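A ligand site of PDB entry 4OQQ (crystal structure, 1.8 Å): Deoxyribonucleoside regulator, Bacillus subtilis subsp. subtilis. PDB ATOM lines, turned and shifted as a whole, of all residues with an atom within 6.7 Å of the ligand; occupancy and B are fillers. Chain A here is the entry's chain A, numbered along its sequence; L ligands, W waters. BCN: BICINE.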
ATOM      1  N   TYR A  38      31.211   6.448   1.931  1.00  0.00           N
ATOM      2  CA  TYR A  38      30.552   6.966   0.711  1.00  0.00           C
ATOM      3  C   TYR A  38      29.494   6.018   0.159  1.00  0.00           C
ATOM      4  O   TYR A  38      28.387   6.456  -0.177  1.00  0.00           O
ATOM      5  CB  TYR A  38      31.559   7.298  -0.392  1.00  0.00           C
ATOM      6  CG  TYR A  38      30.901   7.973  -1.602  1.00  0.00           C
ATOM      7  CD1 TYR A  38      30.446   9.305  -1.523  1.00  0.00           C
ATOM      8  CD2 TYR A  38      30.689   7.283  -2.793  1.00  0.00           C
ATOM      9  CE1 TYR A  38      29.823   9.921  -2.615  1.00  0.00           C
ATOM     10  CE2 TYR A  38      30.083   7.873  -3.879  1.00  0.00           C
ATOM     11  CZ  TYR A  38      29.648   9.195  -3.780  1.00  0.00           C
ATOM     12  OH  TYR A  38      29.036   9.775  -4.860  1.00  0.00           O
ATOM     13  N   THR A  42      25.560   6.606  -0.402  1.00  0.00           N
ATOM     14  CA  THR A  42      25.059   6.576  -1.788  1.00  0.00           C
ATOM     15  C   THR A  42      23.861   5.654  -1.949  1.00  0.00           C
ATOM     16  O   THR A  42      22.882   6.040  -2.580  1.00  0.00           O
ATOM     17  CB  THR A  42      26.184   6.278  -2.812  1.00  0.00           C
ATOM     18  OG1 THR A  42      27.144   7.335  -2.756  1.00  0.00           O
ATOM     19  CG2 THR A  42      25.644   6.218  -4.251  1.00  0.00           C
ATOM     20  N   TRP A  67      23.376  12.292 -15.863  1.00  0.00           N
ATOM     21  CA  TRP A  67      24.062  11.017 -15.782  1.00  0.00           C
ATOM     22  C   TRP A  67      25.247  11.107 -14.836  1.00  0.00           C
ATOM     23  O   TRP A  67      25.786  12.203 -14.598  1.00  0.00           O
ATOM     24  CB  TRP A  67      24.560  10.521 -17.137  1.00  0.00           C
ATOM     25  CG  TRP A  67      25.391  11.446 -17.963  1.00  0.00           C
ATOM     26  CD1 TRP A  67      24.955  12.316 -18.955  1.00  0.00           C
ATOM     27  CD2 TRP A  67      26.823  11.582 -17.955  1.00  0.00           C
ATOM     28  NE1 TRP A  67      26.011  12.968 -19.519  1.00  0.00           N
ATOM     29  CE2 TRP A  67      27.167  12.523 -18.956  1.00  0.00           C
ATOM     30  CE3 TRP A  67      27.846  10.971 -17.217  1.00  0.00           C
ATOM     31  CZ2 TRP A  67      28.470  12.895 -19.204  1.00  0.00           C
ATOM     32  CZ3 TRP A  67      29.146  11.327 -17.480  1.00  0.00           C
ATOM     33  CH2 TRP A  67      29.445  12.287 -18.451  1.00  0.00           C
ATOM     34  N   GLY A  68      25.658   9.938 -14.343  1.00  0.00           N
ATOM     35  CA  GLY A  68      26.749   9.805 -13.393  1.00  0.00           C
ATOM     36  C   GLY A  68      26.429   8.599 -12.512  1.00  0.00           C
ATOM     37  O   GLY A  68      25.334   8.061 -12.569  1.00  0.00           O
ATOM     38  N   THR A  69      27.348   8.221 -11.647  1.00  0.00           N
ATOM     39  CA  THR A  69      27.163   6.996 -10.872  1.00  0.00           C
ATOM     40  C   THR A  69      25.942   7.126  -9.935  1.00  0.00           C
ATOM     41  O   THR A  69      25.077   6.275  -9.920  1.00  0.00           O
ATOM     42  CB  THR A  69      28.435   6.635 -10.099  1.00  0.00           C
ATOM     43  OG1 THR A  69      28.800   7.731  -9.265  1.00  0.00           O
ATOM     44  CG2 THR A  69      29.594   6.335 -11.065  1.00  0.00           C
ATOM     45  N   THR A  70      25.841   8.212  -9.180  1.00  0.00           N
ATOM     46  CA  THR A  70      24.665   8.366  -8.338  1.00  0.00           C
ATOM     47  C   THR A  70      23.358   8.350  -9.126  1.00  0.00           C
ATOM     48  O   THR A  70      22.411   7.633  -8.777  1.00  0.00           O
ATOM     49  CB  THR A  70      24.785   9.641  -7.478  1.00  0.00           C
ATOM     50  OG1 THR A  70      25.964   9.512  -6.685  1.00  0.00           O
ATOM     51  CG2 THR A  70      23.568   9.777  -6.556  1.00  0.00           C
ATOM     52  N   MET A  71      23.307   9.106 -10.233  1.00  0.00           N
ATOM     53  CA  MET A  71      22.095   9.133 -11.038  1.00  0.00           C
ATOM     54  C   MET A  71      21.701   7.736 -11.546  1.00  0.00           C
ATOM     55  O   MET A  71      20.513   7.390 -11.543  1.00  0.00           O
ATOM     56  CB  MET A  71      22.273  10.144 -12.209  1.00  0.00           C
ATOM     57  CG  MET A  71      22.305  11.610 -11.735  1.00  0.00           C
ATOM     58  SD  MET A  71      20.742  12.149 -10.978  1.00  0.00           S
ATOM     59  CE  MET A  71      19.626  11.952 -12.358  1.00  0.00           C
ATOM     60  N   TYR A  72      22.699   6.940 -11.965  1.00  0.00           N
ATOM     61  CA  TYR A  72      22.460   5.571 -12.457  1.00  0.00           C
ATOM     62  C   TYR A  72      21.847   4.706 -11.389  1.00  0.00           C
ATOM     63  O   TYR A  72      20.904   3.964 -11.659  1.00  0.00           O
ATOM     64  CB  TYR A  72      23.781   4.935 -12.907  1.00  0.00           C
ATOM     65  CG  TYR A  72      23.644   3.554 -13.554  1.00  0.00           C
ATOM     66  CD1 TYR A  72      22.558   3.245 -14.391  1.00  0.00           C
ATOM     67  CD2 TYR A  72      24.626   2.583 -13.352  1.00  0.00           C
ATOM     68  CE1 TYR A  72      22.445   2.000 -14.980  1.00  0.00           C
ATOM     69  CE2 TYR A  72      24.525   1.330 -13.942  1.00  0.00           C
ATOM     70  CZ  TYR A  72      23.448   1.048 -14.772  1.00  0.00           C
ATOM     71  OH  TYR A  72      23.359  -0.189 -15.327  1.00  0.00           O
ATOM     72  N   LYS A  92      22.461  16.954 -19.458  1.00  0.00           N
ATOM     73  CA  LYS A  92      23.899  16.918 -19.445  1.00  0.00           C
ATOM     74  C   LYS A  92      24.486  16.399 -20.752  1.00  0.00           C
ATOM     75  O   LYS A  92      23.984  15.450 -21.330  1.00  0.00           O
ATOM     76  CB  LYS A  92      24.301  16.070 -18.233  1.00  0.00           C
ATOM     77  CG  LYS A  92      25.778  16.113 -17.960  1.00  0.00           C
ATOM     78  CD  LYS A  92      26.105  15.291 -16.734  1.00  0.00           C
ATOM     79  CE  LYS A  92      27.617  15.113 -16.592  1.00  0.00           C
ATOM     80  NZ  LYS A  92      27.855  14.410 -15.297  1.00  0.00           N
ATOM     81  N   THR A 102      29.618   5.440 -18.571  1.00  0.00           N
ATOM     82  CA  THR A 102      28.826   6.482 -17.896  1.00  0.00           C
ATOM     83  C   THR A 102      27.390   6.042 -17.573  1.00  0.00           C
ATOM     84  O   THR A 102      26.696   6.663 -16.710  1.00  0.00           O
ATOM     85  CB  THR A 102      28.752   7.767 -18.725  1.00  0.00           C
ATOM     86  OG1 THR A 102      27.999   7.517 -19.928  1.00  0.00           O
ATOM     87  CG2 THR A 102      30.149   8.277 -19.065  1.00  0.00           C
ATOM     88  N   THR A 159      23.094  15.242  -9.214  1.00  0.00           N
ATOM     89  CA  THR A 159      24.041  15.329  -8.106  1.00  0.00           C
ATOM     90  C   THR A 159      25.053  16.451  -8.382  1.00  0.00           C
ATOM     91  O   THR A 159      24.954  17.154  -9.414  1.00  0.00           O
ATOM     92  CB  THR A 159      24.758  13.971  -7.816  1.00  0.00           C
ATOM     93  OG1 THR A 159      25.333  14.002  -6.490  1.00  0.00           O
ATOM     94  CG2 THR A 159      25.847  13.663  -8.904  1.00  0.00           C
ATOM     95  N   VAL A 160      25.983  16.657  -7.459  1.00  0.00           N
ATOM     96  CA  VAL A 160      27.147  17.493  -7.740  1.00  0.00           C
ATOM     97  C   VAL A 160      28.373  16.624  -7.894  1.00  0.00           C
ATOM     98  O   VAL A 160      28.497  15.585  -7.224  1.00  0.00           O
ATOM     99  CB  VAL A 160      27.419  18.569  -6.659  1.00  0.00           C
ATOM    100  CG1 VAL A 160      26.349  19.651  -6.686  1.00  0.00           C
ATOM    101  CG2 VAL A 160      27.577  17.980  -5.251  1.00  0.00           C
ATOM    102  N   GLY A 161      29.268  17.029  -8.786  1.00  0.00           N
ATOM    103  CA  GLY A 161      30.586  16.403  -8.918  1.00  0.00           C
ATOM    104  C   GLY A 161      31.638  17.213  -8.189  1.00  0.00           C
ATOM    105  O   GLY A 161      31.412  18.357  -7.829  1.00  0.00           O
ATOM    106  N   THR A 162      32.784  16.606  -7.928  1.00  0.00           N
ATOM    107  CA  THR A 162      33.856  17.320  -7.243  1.00  0.00           C
ATOM    108  C   THR A 162      34.959  17.737  -8.210  1.00  0.00           C
ATOM    109  O   THR A 162      34.879  17.417  -9.392  1.00  0.00           O
ATOM    110  CB  THR A 162      34.441  16.461  -6.122  1.00  0.00           C
ATOM    111  OG1 THR A 162      35.012  15.292  -6.689  1.00  0.00           O
ATOM    112  CG2 THR A 162      33.365  16.045  -5.141  1.00  0.00           C
ATOM    113  N   VAL A 163      35.974  18.441  -7.696  1.00  0.00           N
ATOM    114  CA  VAL A 163      37.143  18.857  -8.502  1.00  0.00           C
ATOM    115  C   VAL A 163      38.451  18.092  -8.169  1.00  0.00           C
ATOM    116  O   VAL A 163      39.556  18.594  -8.317  1.00  0.00           O
ATOM    117  CB  VAL A 163      37.361  20.393  -8.431  1.00  0.00           C
ATOM    118  CG1 VAL A 163      36.139  21.098  -8.949  1.00  0.00           C
ATOM    119  CG2 VAL A 163      37.691  20.873  -7.027  1.00  0.00           C
ATOM    120  N   ARG A 164      38.336  16.846  -7.739  1.00  0.00           N
ATOM    121  CA  ARG A 164      39.538  16.042  -7.525  1.00  0.00           C
ATOM    122  C   ARG A 164      40.325  15.779  -8.829  1.00  0.00           C
ATOM    123  O   ARG A 164      39.752  15.783  -9.896  1.00  0.00           O
ATOM    124  CB  ARG A 164      39.141  14.712  -6.907  1.00  0.00           C
ATOM    125  CG  ARG A 164      38.307  14.815  -5.642  1.00  0.00           C
ATOM    126  CD  ARG A 164      37.788  13.432  -5.268  1.00  0.00           C
ATOM    127  NE  ARG A 164      37.022  12.830  -6.368  1.00  0.00           N
ATOM    128  CZ  ARG A 164      36.773  11.524  -6.508  1.00  0.00           C
ATOM    129  NH1 ARG A 164      37.218  10.647  -5.607  1.00  0.00           N
ATOM    130  NH2 ARG A 164      36.069  11.103  -7.549  1.00  0.00           N
ATOM    131  N   ALA A 167      38.621  13.572 -11.376  1.00  0.00           N
ATOM    132  CA  ALA A 167      37.354  13.969 -12.017  1.00  0.00           C
ATOM    133  C   ALA A 167      37.437  13.714 -13.499  1.00  0.00           C
ATOM    134  O   ALA A 167      38.450  14.075 -14.171  1.00  0.00           O
ATOM    135  CB  ALA A 167      37.014  15.438 -11.763  1.00  0.00           C
ATOM    136  N   LEU A 168      36.354  13.153 -14.019  1.00  0.00           N
ATOM    137  CA  LEU A 168      36.248  12.798 -15.440  1.00  0.00           C
ATOM    138  C   LEU A 168      36.627  13.942 -16.359  1.00  0.00           C
ATOM    139  O   LEU A 168      37.430  13.767 -17.295  1.00  0.00           O
ATOM    140  CB  LEU A 168      34.828  12.351 -15.726  1.00  0.00           C
ATOM    141  CG  LEU A 168      34.543  11.848 -17.135  1.00  0.00           C
ATOM    142  CD1 LEU A 168      35.420  10.656 -17.520  1.00  0.00           C
ATOM    143  CD2 LEU A 168      33.089  11.472 -17.154  1.00  0.00           C
ATOM    144  N   ASP A 190      30.774  20.822  -9.848  1.00  0.00           N
ATOM    145  CA  ASP A 190      30.014  21.006 -11.092  1.00  0.00           C
ATOM    146  C   ASP A 190      28.618  20.470 -10.923  1.00  0.00           C
ATOM    147  O   ASP A 190      28.414  19.478 -10.187  1.00  0.00           O
ATOM    148  CB  ASP A 190      30.673  20.331 -12.308  1.00  0.00           C
ATOM    149  CG  ASP A 190      30.406  18.800 -12.388  1.00  0.00           C
ATOM    150  OD1 ASP A 190      31.066  18.044 -11.635  1.00  0.00           O
ATOM    151  OD2 ASP A 190      29.572  18.343 -13.198  1.00  0.00           O
ATOM    152  N   VAL A 228      20.578  15.451  -5.062  1.00  0.00           N
ATOM    153  CA  VAL A 228      20.809  14.276  -4.209  1.00  0.00           C
ATOM    154  C   VAL A 228      22.312  14.189  -4.081  1.00  0.00           C
ATOM    155  O   VAL A 228      23.012  14.028  -5.080  1.00  0.00           O
ATOM    156  CB  VAL A 228      20.344  12.991  -4.903  1.00  0.00           C
ATOM    157  CG1 VAL A 228      20.568  11.790  -4.024  1.00  0.00           C
ATOM    158  CG2 VAL A 228      18.866  13.110  -5.281  1.00  0.00           C
ATOM    159  N   ALA A 229      22.809  14.343  -2.875  1.00  0.00           N
ATOM    160  CA  ALA A 229      24.261  14.303  -2.693  1.00  0.00           C
ATOM    161  C   ALA A 229      24.587  14.098  -1.237  1.00  0.00           C
ATOM    162  O   ALA A 229      23.851  14.565  -0.372  1.00  0.00           O
ATOM    163  CB  ALA A 229      24.897  15.601  -3.161  1.00  0.00           C
ATOM    164  N   GLY A 230      25.748  13.477  -0.998  1.00  0.00           N
ATOM    165  CA  GLY A 230      26.295  13.309   0.345  1.00  0.00           C
ATOM    166  C   GLY A 230      27.682  12.680   0.305  1.00  0.00           C
ATOM    167  O   GLY A 230      28.116  12.180  -0.752  1.00  0.00           O
ATOM    168  N   ARG A 233      33.502  13.931   0.975  1.00  0.00           N
ATOM    169  CA  ARG A 233      34.176  14.334  -0.277  1.00  0.00           C
ATOM    170  C   ARG A 233      33.450  15.479  -1.019  1.00  0.00           C
ATOM    171  O   ARG A 233      34.053  16.243  -1.800  1.00  0.00           O
ATOM    172  CB  ARG A 233      34.280  13.067  -1.147  1.00  0.00           C
ATOM    173  CG  ARG A 233      34.764  13.204  -2.594  1.00  0.00           C
ATOM    174  CD  ARG A 233      34.895  11.849  -3.297  1.00  0.00           C
ATOM    175  NE  ARG A 233      33.933  11.660  -4.401  1.00  0.00           N
ATOM    176  CZ  ARG A 233      33.107  10.623  -4.545  1.00  0.00           C
ATOM    177  NH1 ARG A 233      32.288  10.571  -5.596  1.00  0.00           N
ATOM    178  NH2 ARG A 233      33.075   9.637  -3.652  1.00  0.00           N
ATOM    179  N   LYS A 234      32.142  15.590  -0.765  1.00  0.00           N
ATOM    180  CA  LYS A 234      31.281  16.503  -1.497  1.00  0.00           C
ATOM    181  C   LYS A 234      30.783  17.673  -0.669  1.00  0.00           C
ATOM    182  O   LYS A 234      29.973  18.448  -1.139  1.00  0.00           O
ATOM    183  CB  LYS A 234      30.080  15.720  -2.017  1.00  0.00           C
ATOM    184  CG  LYS A 234      30.405  14.705  -3.107  1.00  0.00           C
ATOM    185  CD  LYS A 234      29.135  14.355  -3.875  1.00  0.00           C
ATOM    186  CE  LYS A 234      29.423  13.448  -5.070  1.00  0.00           C
ATOM    187  NZ  LYS A 234      28.147  13.011  -5.671  1.00  0.00           N
HETATM  188  N1  BCN L   1      30.299  11.804  -9.510  1.00  0.00           N
HETATM  189  C1  BCN L   1      29.822  10.949  -8.400  1.00  0.00           C
HETATM  190  C2  BCN L   1      28.309  10.853  -8.352  1.00  0.00           C
HETATM  191  O21 BCN L   1      27.577  10.553  -9.335  1.00  0.00           O
HETATM  192  O22 BCN L   1      27.772  11.061  -7.257  1.00  0.00           O
HETATM  193  C3  BCN L   1      31.760  11.978  -9.415  1.00  0.00           C
HETATM  194  C4  BCN L   1      32.052  13.091  -8.404  1.00  0.00           C
HETATM  195  O4  BCN L   1      33.283  13.733  -8.701  1.00  0.00           O
HETATM  196  C5  BCN L   1      29.928  11.308 -10.860  1.00  0.00           C
HETATM  197  C6  BCN L   1      30.540   9.964 -11.203  1.00  0.00           C
HETATM  198  O6  BCN L   1      29.778   9.434 -12.291  1.00  0.00           O
HETATM  199  O   HOH W   1      28.322  13.689 -11.315  1.00  0.00           O
HETATM  200  O   HOH W   2      25.168  11.046 -10.767  1.00  0.00           O
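Water W2 lies within hydrogen-bond range of N of Met 71 (2.7 Å), O21 of the ligand (2.8 Å), N of Thr 70 (3.3 Å) and O of Gly 68 (3.5 Å).
The backbone NH (N) of Thr 70 lies within hydrogen-bond range of an oxygen (O21) of the ligand, at 2.9 Å. The side-chain hydroxyl (OG1) of Thr 70 sits at hydrogen-bond distance from an oxygen (O22) of the ligand. An oxygen (O22) of the ligand is in salt-bridge range of the side-chain amino group (NZ) of Lys 234 (2.5 Å). The backbone NH (N) of Thr 69 sits at hydrogen-bond distance from an oxygen (O6) of the ligand (2.8 Å). The side-chain hydroxyl of Thr 69 is in hydrogen-bond range of an oxygen (O21) of the ligand (3.1 Å). An oxygen (O22) of the ligand sits at hydrogen-bond distance from the side-chain hydroxyl (OH) of Tyr 38 (3.0 Å). The backbone NH (N) of Thr 162 lies within hydrogen-bond range of an oxygen (O4) of the ligand, 3.0 Å away. The side-chain hydroxyl of Thr 162 lies within hydrogen-bond range of an oxygen (O4) of the ligand (3.1 Å).
The side-chain amino group (NZ) of Lys 234 sits at hydrogen-bond distance from the side-chain hydroxyl (OH) of Tyr 38, at 3.5 Å. The side-chain amino group (NZ) of Lys 234 is in hydrogen-bond range of the side-chain hydroxyl (OG1) of Thr 159, at 3.1 Å. The backbone carbonyl oxygen (O) of Val 160 is in hydrogen-bond range of the side-chain amino group (NZ) of Lys 234 (3.0 Å). OH of Tyr 38 sits at hydrogen-bond distance from NH1 of Arg 233, at 3.4 Å. The backbone carbonyl oxygen (O) of Tyr 38 sits at hydrogen-bond distance from the side-chain hydroxyl (OG1) of Thr 42. OG1 of Thr 162 sits at hydrogen-bond distance from NE of Arg 164 (3.2 Å). The side-chain hydroxyl (OG1) of Thr 159 sits at hydrogen-bond distance from the backbone carbonyl oxygen (O) of Val 228, at 2.7 Å. N of Gly 161 sits at hydrogen-bond distance from O of Asp 190, at 2.9 Å.
CA of Gly 68 touches O6 of the ligand, at 3.2 Å. CG2 of Thr 159 touches O21 of the ligand, 3.6 Å away. Gly 161 touches the ligand (CA to C4, 3.7 Å). Arg 233 touches the ligand. Of the 24 residues printed, 9 come within 4 Å of the ligand. The nearest printed residue that does not touch the ligand is Arg 164 (4.001 Å).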
